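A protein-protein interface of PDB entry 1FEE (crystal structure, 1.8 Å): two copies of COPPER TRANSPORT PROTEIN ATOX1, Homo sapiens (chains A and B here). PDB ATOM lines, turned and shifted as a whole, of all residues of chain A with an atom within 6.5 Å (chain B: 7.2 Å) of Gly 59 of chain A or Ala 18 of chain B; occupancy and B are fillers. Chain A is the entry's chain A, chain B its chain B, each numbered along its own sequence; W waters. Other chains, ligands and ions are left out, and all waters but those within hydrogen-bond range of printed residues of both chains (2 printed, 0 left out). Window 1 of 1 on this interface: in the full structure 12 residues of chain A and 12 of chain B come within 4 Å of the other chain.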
ATOM      1  N   LEU A  55       2.131  -6.656  22.963  1.00  0.00           N
ATOM      2  CA  LEU A  55       2.434  -6.059  21.662  1.00  0.00           C
ATOM      3  C   LEU A  55       2.554  -4.539  21.732  1.00  0.00           C
ATOM      4  O   LEU A  55       3.414  -3.951  21.078  1.00  0.00           O
ATOM      5  CB  LEU A  55       1.369  -6.448  20.632  1.00  0.00           C
ATOM      6  CG  LEU A  55       1.324  -7.928  20.228  1.00  0.00           C
ATOM      7  CD1 LEU A  55       0.116  -8.187  19.337  1.00  0.00           C
ATOM      8  CD2 LEU A  55       2.611  -8.303  19.504  1.00  0.00           C
ATOM      9  N   LYS A  56       1.702  -3.895  22.524  1.00  0.00           N
ATOM     10  CA  LYS A  56       1.748  -2.440  22.635  1.00  0.00           C
ATOM     11  C   LYS A  56       2.991  -1.923  23.352  1.00  0.00           C
ATOM     12  O   LYS A  56       3.404  -0.786  23.135  1.00  0.00           O
ATOM     13  CB  LYS A  56       0.494  -1.911  23.340  1.00  0.00           C
ATOM     14  CG  LYS A  56      -0.752  -1.910  22.465  1.00  0.00           C
ATOM     15  CD  LYS A  56      -1.941  -1.311  23.201  1.00  0.00           C
ATOM     16  CE  LYS A  56      -3.168  -1.213  22.302  1.00  0.00           C
ATOM     17  NZ  LYS A  56      -2.960  -0.286  21.155  1.00  0.00           N
ATOM     18  N   LYS A  57       3.590  -2.755  24.198  1.00  0.00           N
ATOM     19  CA  LYS A  57       4.786  -2.347  24.927  1.00  0.00           C
ATOM     20  C   LYS A  57       5.980  -2.110  24.008  1.00  0.00           C
ATOM     21  O   LYS A  57       6.929  -1.426  24.387  1.00  0.00           O
ATOM     22  CB  LYS A  57       5.152  -3.387  25.990  1.00  0.00           C
ATOM     23  CG  LYS A  57       4.227  -3.389  27.194  1.00  0.00           C
ATOM     24  CD  LYS A  57       4.718  -4.341  28.272  1.00  0.00           C
ATOM     25  CE  LYS A  57       3.809  -4.304  29.491  1.00  0.00           C
ATOM     26  NZ  LYS A  57       4.275  -5.227  30.563  1.00  0.00           N
ATOM     27  N   THR A  58       5.923  -2.666  22.802  1.00  0.00           N
ATOM     28  CA  THR A  58       7.002  -2.520  21.826  1.00  0.00           C
ATOM     29  C   THR A  58       7.095  -1.114  21.244  1.00  0.00           C
ATOM     30  O   THR A  58       8.095  -0.760  20.619  1.00  0.00           O
ATOM     31  CB  THR A  58       6.816  -3.463  20.635  1.00  0.00           C
ATOM     32  OG1 THR A  58       5.619  -3.100  19.932  1.00  0.00           O
ATOM     33  CG2 THR A  58       6.733  -4.912  21.098  1.00  0.00           C
ATOM     34  N   GLY A  59       6.046  -0.323  21.430  1.00  0.00           N
ATOM     35  CA  GLY A  59       6.043   1.024  20.895  1.00  0.00           C
ATOM     36  C   GLY A  59       5.489   1.081  19.481  1.00  0.00           C
ATOM     37  O   GLY A  59       5.455   2.144  18.863  1.00  0.00           O
ATOM     38  N   LYS A  60       5.058  -0.064  18.957  1.00  0.00           N
ATOM     39  CA  LYS A  60       4.494  -0.111  17.611  1.00  0.00           C
ATOM     40  C   LYS A  60       2.981   0.092  17.677  1.00  0.00           C
ATOM     41  O   LYS A  60       2.363  -0.133  18.720  1.00  0.00           O
ATOM     42  CB  LYS A  60       4.808  -1.457  16.948  1.00  0.00           C
ATOM     43  CG  LYS A  60       6.298  -1.762  16.860  1.00  0.00           C
ATOM     44  CD  LYS A  60       6.581  -2.981  15.991  1.00  0.00           C
ATOM     45  CE  LYS A  60       8.050  -3.392  16.079  1.00  0.00           C
ATOM     46  NZ  LYS A  60       8.978  -2.264  15.781  1.00  0.00           N
ATOM     47  N   THR A  61       2.394   0.529  16.569  1.00  0.00           N
ATOM     48  CA  THR A  61       0.952   0.751  16.513  1.00  0.00           C
ATOM     49  C   THR A  61       0.263  -0.604  16.376  1.00  0.00           C
ATOM     50  O   THR A  61       0.537  -1.353  15.437  1.00  0.00           O
ATOM     51  CB  THR A  61       0.583   1.653  15.322  1.00  0.00           C
ATOM     52  OG1 THR A  61       1.263   2.908  15.452  1.00  0.00           O
ATOM     53  CG2 THR A  61      -0.917   1.909  15.289  1.00  0.00           C
ATOM     54  N   CYS B  12      14.861   0.635  10.322  1.00  0.00           N
ATOM     55  CA  CYS B  12      13.952   1.418   9.486  1.00  0.00           C
ATOM     56  C   CYS B  12      13.351   2.559  10.305  1.00  0.00           C
ATOM     57  O   CYS B  12      13.489   2.590  11.530  1.00  0.00           O
ATOM     58  CB  CYS B  12      12.833   0.537   8.901  1.00  0.00           C
ATOM     59  SG  CYS B  12      11.373   0.291   9.947  1.00  0.00           S
ATOM     60  N   GLY B  13      12.694   3.494   9.623  1.00  0.00           N
ATOM     61  CA  GLY B  13      12.080   4.624  10.301  1.00  0.00           C
ATOM     62  C   GLY B  13      11.055   4.187  11.332  1.00  0.00           C
ATOM     63  O   GLY B  13      10.913   4.819  12.381  1.00  0.00           O
ATOM     64  N   GLY B  14      10.336   3.112  11.024  1.00  0.00           N
ATOM     65  CA  GLY B  14       9.337   2.588  11.942  1.00  0.00           C
ATOM     66  C   GLY B  14       9.984   2.117  13.234  1.00  0.00           C
ATOM     67  O   GLY B  14       9.375   2.206  14.304  1.00  0.00           O
ATOM     68  N   CYS B  15      11.208   1.598  13.132  1.00  0.00           N
ATOM     69  CA  CYS B  15      11.962   1.140  14.300  1.00  0.00           C
ATOM     70  C   CYS B  15      12.256   2.352  15.191  1.00  0.00           C
ATOM     71  O   CYS B  15      12.133   2.287  16.417  1.00  0.00           O
ATOM     72  CB  CYS B  15      13.298   0.501  13.882  1.00  0.00           C
ATOM     73  SG  CYS B  15      13.215  -1.135  13.073  1.00  0.00           S
ATOM     74  N   ALA B  16      12.656   3.454  14.562  1.00  0.00           N
ATOM     75  CA  ALA B  16      12.962   4.682  15.289  1.00  0.00           C
ATOM     76  C   ALA B  16      11.713   5.249  15.965  1.00  0.00           C
ATOM     77  O   ALA B  16      11.777   5.719  17.100  1.00  0.00           O
ATOM     78  CB  ALA B  16      13.567   5.722  14.335  1.00  0.00           C
ATOM     79  N   GLU B  17      10.579   5.203  15.271  1.00  0.00           N
ATOM     80  CA  GLU B  17       9.333   5.715  15.841  1.00  0.00           C
ATOM     81  C   GLU B  17       8.945   4.923  17.086  1.00  0.00           C
ATOM     82  O   GLU B  17       8.472   5.496  18.070  1.00  0.00           O
ATOM     83  CB  GLU B  17       8.197   5.645  14.814  1.00  0.00           C
ATOM     84  CG  GLU B  17       8.423   6.486  13.562  1.00  0.00           C
ATOM     85  CD  GLU B  17       7.329   6.289  12.527  1.00  0.00           C
ATOM     86  OE1 GLU B  17       6.720   5.196  12.503  1.00  0.00           O
ATOM     87  OE2 GLU B  17       7.088   7.215  11.723  1.00  0.00           O
ATOM     88  N   ALA B  18       9.147   3.607  17.046  1.00  0.00           N
ATOM     89  CA  ALA B  18       8.813   2.751  18.183  1.00  0.00           C
ATOM     90  C   ALA B  18       9.663   3.112  19.398  1.00  0.00           C
ATOM     91  O   ALA B  18       9.161   3.165  20.521  1.00  0.00           O
ATOM     92  CB  ALA B  18       9.014   1.275  17.814  1.00  0.00           C
ATOM     93  N   VAL B  19      10.953   3.349  19.173  1.00  0.00           N
ATOM     94  CA  VAL B  19      11.856   3.728  20.259  1.00  0.00           C
ATOM     95  C   VAL B  19      11.349   5.048  20.842  1.00  0.00           C
ATOM     96  O   VAL B  19      11.296   5.233  22.063  1.00  0.00           O
ATOM     97  CB  VAL B  19      13.301   3.906  19.739  1.00  0.00           C
ATOM     98  CG1 VAL B  19      14.174   4.549  20.812  1.00  0.00           C
ATOM     99  CG2 VAL B  19      13.869   2.548  19.327  1.00  0.00           C
ATOM    100  N   SER B  20      10.965   5.965  19.961  1.00  0.00           N
ATOM    101  CA  SER B  20      10.443   7.250  20.406  1.00  0.00           C
ATOM    102  C   SER B  20       9.206   7.066  21.289  1.00  0.00           C
ATOM    103  O   SER B  20       9.082   7.697  22.341  1.00  0.00           O
ATOM    104  CB  SER B  20      10.076   8.117  19.203  1.00  0.00           C
ATOM    105  OG  SER B  20       9.418   9.294  19.629  1.00  0.00           O
ATOM    106  N   ARG B  21       8.290   6.203  20.864  1.00  0.00           N
ATOM    107  CA  ARG B  21       7.079   5.978  21.646  1.00  0.00           C
ATOM    108  C   ARG B  21       7.334   5.404  23.043  1.00  0.00           C
ATOM    109  O   ARG B  21       6.703   5.838  24.005  1.00  0.00           O
ATOM    110  CB  ARG B  21       6.098   5.075  20.888  1.00  0.00           C
ATOM    111  CG  ARG B  21       5.544   5.693  19.614  1.00  0.00           C
ATOM    112  CD  ARG B  21       4.191   5.094  19.241  1.00  0.00           C
ATOM    113  NE  ARG B  21       3.730   5.556  17.935  1.00  0.00           N
ATOM    114  CZ  ARG B  21       4.101   5.020  16.774  1.00  0.00           C
ATOM    115  NH1 ARG B  21       4.941   3.992  16.746  1.00  0.00           N
ATOM    116  NH2 ARG B  21       3.646   5.524  15.635  1.00  0.00           N
ATOM    117  N   VAL B  22       8.242   4.436  23.173  1.00  0.00           N
ATOM    118  CA  VAL B  22       8.498   3.875  24.500  1.00  0.00           C
ATOM    119  C   VAL B  22       9.168   4.905  25.410  1.00  0.00           C
ATOM    120  O   VAL B  22       8.907   4.935  26.612  1.00  0.00           O
ATOM    121  CB  VAL B  22       9.367   2.576  24.455  1.00  0.00           C
ATOM    122  CG1 VAL B  22       8.697   1.537  23.569  1.00  0.00           C
ATOM    123  CG2 VAL B  22      10.773   2.880  23.966  1.00  0.00           C
ATOM    124  N   LEU B  23      10.013   5.762  24.843  1.00  0.00           N
ATOM    125  CA  LEU B  23      10.679   6.787  25.644  1.00  0.00           C
ATOM    126  C   LEU B  23       9.683   7.885  26.020  1.00  0.00           C
ATOM    127  O   LEU B  23       9.726   8.421  27.128  1.00  0.00           O
ATOM    128  CB  LEU B  23      11.870   7.373  24.880  1.00  0.00           C
ATOM    129  CG  LEU B  23      13.027   6.383  24.675  1.00  0.00           C
ATOM    130  CD1 LEU B  23      14.133   7.037  23.863  1.00  0.00           C
ATOM    131  CD2 LEU B  23      13.565   5.931  26.032  1.00  0.00           C
ATOM    132  N   ASN B  24       8.783   8.215  25.099  1.00  0.00           N
ATOM    133  CA  ASN B  24       7.763   9.230  25.371  1.00  0.00           C
ATOM    134  C   ASN B  24       6.884   8.754  26.525  1.00  0.00           C
ATOM    135  O   ASN B  24       6.500   9.539  27.395  1.00  0.00           O
ATOM    136  CB  ASN B  24       6.878   9.456  24.140  1.00  0.00           C
ATOM    137  CG  ASN B  24       7.542  10.321  23.080  1.00  0.00           C
ATOM    138  OD1 ASN B  24       7.020  10.470  21.974  1.00  0.00           O
ATOM    139  ND2 ASN B  24       8.687  10.903  23.413  1.00  0.00           N
ATOM    140  N   ILE B  33      17.734  10.317  18.496  1.00  0.00           N
ATOM    141  CA  ILE B  33      17.860   9.022  17.825  1.00  0.00           C
ATOM    142  C   ILE B  33      18.605   9.161  16.499  1.00  0.00           C
ATOM    143  O   ILE B  33      18.204   9.933  15.633  1.00  0.00           O
ATOM    144  CB  ILE B  33      16.454   8.412  17.569  1.00  0.00           C
ATOM    145  CG1 ILE B  33      15.767   8.116  18.908  1.00  0.00           C
ATOM    146  CG2 ILE B  33      16.561   7.142  16.729  1.00  0.00           C
ATOM    147  CD1 ILE B  33      14.261   7.868  18.791  1.00  0.00           C
ATOM    148  N   LYS B  57      12.059  -2.945  25.908  1.00  0.00           N
ATOM    149  CA  LYS B  57      10.645  -3.255  25.696  1.00  0.00           C
ATOM    150  C   LYS B  57      10.292  -3.254  24.210  1.00  0.00           C
ATOM    151  O   LYS B  57       9.291  -3.842  23.800  1.00  0.00           O
ATOM    152  CB  LYS B  57       9.752  -2.252  26.433  1.00  0.00           C
ATOM    153  CG  LYS B  57       9.796  -2.371  27.948  1.00  0.00           C
ATOM    154  CD  LYS B  57       8.919  -1.319  28.613  1.00  0.00           C
ATOM    155  CE  LYS B  57       8.957  -1.461  30.131  1.00  0.00           C
ATOM    156  NZ  LYS B  57       8.157  -0.409  30.819  1.00  0.00           N
ATOM    157  N   THR B  58      11.112  -2.590  23.403  1.00  0.00           N
ATOM    158  CA  THR B  58      10.871  -2.528  21.964  1.00  0.00           C
ATOM    159  C   THR B  58      11.078  -3.895  21.323  1.00  0.00           C
ATOM    160  O   THR B  58      10.584  -4.152  20.229  1.00  0.00           O
ATOM    161  CB  THR B  58      11.836  -1.562  21.260  1.00  0.00           C
ATOM    162  OG1 THR B  58      13.182  -2.008  21.470  1.00  0.00           O
ATOM    163  CG2 THR B  58      11.668  -0.145  21.784  1.00  0.00           C
ATOM    164  N   LYS B  60      13.991  -4.893  20.520  1.00  0.00           N
ATOM    165  CA  LYS B  60      15.204  -4.738  19.723  1.00  0.00           C
ATOM    166  C   LYS B  60      16.424  -5.026  20.593  1.00  0.00           C
ATOM    167  O   LYS B  60      16.347  -4.956  21.819  1.00  0.00           O
ATOM    168  CB  LYS B  60      15.299  -3.313  19.171  1.00  0.00           C
ATOM    169  CG  LYS B  60      14.148  -2.902  18.261  1.00  0.00           C
ATOM    170  CD  LYS B  60      14.308  -1.451  17.841  1.00  0.00           C
ATOM    171  CE  LYS B  60      13.193  -0.993  16.916  1.00  0.00           C
ATOM    172  NZ  LYS B  60      11.854  -1.065  17.552  1.00  0.00           N
HETATM  173  O   HOH W   1      11.505  -2.701  15.460  1.00  0.00           O
HETATM  174  O   HOH W   2       9.604  -1.991  18.780  1.00  0.00           O
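Printed residues of chain A that touch a printed residue of chain B: Lys 57, Thr 58, Gly 59, Lys 60 and Thr 61. Printed residues of chain B that touch a printed residue of chain A: Ala 18, Arg 21, Val 22, Lys 57, Thr 58 and Lys 60. Hydrophobic or aromatic side chains of chain B that line the printed part of chain A: Ala 18 and Val 22. Among the printed residues, 11 pairs touch across the chains. Among the printed residues, no Asp or Glu carboxylate lies within 4 Å of a Lys or Arg side-chain nitrogen of the other chain.
Lys 57 of chain B touches its own counterpart, Lys 57 of chain A. Thr 58 of chain A touches Lys 57 of chain B, but with the chains exchanged Lys 57 of chain A does not touch Thr 58 of chain B (4.5 Å). Thr 58 of chain A touches its own counterpart, Thr 58 of chain B. Lys 60 of chain A touches its own counterpart, Lys 60 of chain B. Of the 11 pairs that touch across the chains among the printed residues, 3 have their exchanged pair printed and touching as well.
Of the printed residues of chain B, Gly 59 of chain A touches Ala 18 (3.5 Å), Arg 21 (2.9 Å) and Val 22 (3.8 Å). Ala 18 of chain B touches just these residues of chain A: Thr 58 (3.6 Å) and Gly 59 (3.5 Å). Of the printed residues of chain A, Lys 60 of chain B touches Lys 60. Of the printed residues of chain A, Thr 58 of chain B touches Thr 58. Of the printed residues of chain B, Lys 57 of chain A touches Val 22 and Lys 57. Printed residues of chain B within 4 Å of Thr 61 of chain A: Arg 21. Printed residues of chain A within 4 Å of Lys 57 of chain B: Lys 57 (3.4 Å) and Thr 58 (3.3 Å). Glu 17 of chain B touches none of the printed residues of chain A. Asn 24 of chain B touches none of the printed residues of chain A.
Water W1 bridges NZ of Lys 60 of chain A and NZ of Lys 60 of chain B. Water W2 lies within hydrogen-bond range of the backbone carbonyl oxygen of Thr 58 of chain A (2.7 Å), the side-chain amino group of Lys 60 of chain B (2.7 Å), the backbone carbonyl oxygen of Thr 58 of chain B (2.8 Å) and the side-chain amino group of Lys 60 of chain A (3.1 Å).
The guanidinium group (NH1) of Arg 21 of chain B lies within hydrogen-bond range of the backbone carbonyl oxygen (O) of Gly 59 of chain A (2.9 Å). The backbone carbonyl oxygen (O) of Lys 57 of chain A lies close to the backbone carbonyl oxygen (O) of Lys 57 of chain B (3.4 Å).
The backbone carbonyl oxygen (O) of Leu 55 of chain A is in hydrogen-bond range of the side-chain hydroxyl (OG1) of Thr 58 of chain A (2.6 Å). The side-chain hydroxyl of Thr 58 of chain A sits close to the backbone NH of Lys 60 of chain A (3.2 Å). The side-chain hydroxyl (OG1) of Thr 58 of chain B sits at hydrogen-bond distance from the backbone NH (N) of Lys 60 of chain B, at 3.1 Å.
Val 22 of chain B touches Lys 57 of chain A. O of Thr 58 of chain A touches CB of Ala 18 of chain B, at 3.6 Å. Val 22 of chain B touches Thr 58 of chain A. Thr 58 of chain A touches Lys 57 of chain B (CA to O, 3.3 Å). O of Thr 58 of chain A touches CA of Thr 58 of chain B (3.6 Å). Ala 18 of chain B touches Gly 59 of chain A (CA to O, 3.5 Å). CG1 of Val 22 of chain B touches CA of Gly 59 of chain A, 3.8 Å away. Lys 60 of chain B touches Lys 60 of chain A (NZ to NZ, 3.6 Å). OG1 of Thr 61 of chain A touches NH2 of Arg 21 of chain B (3.5 Å).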
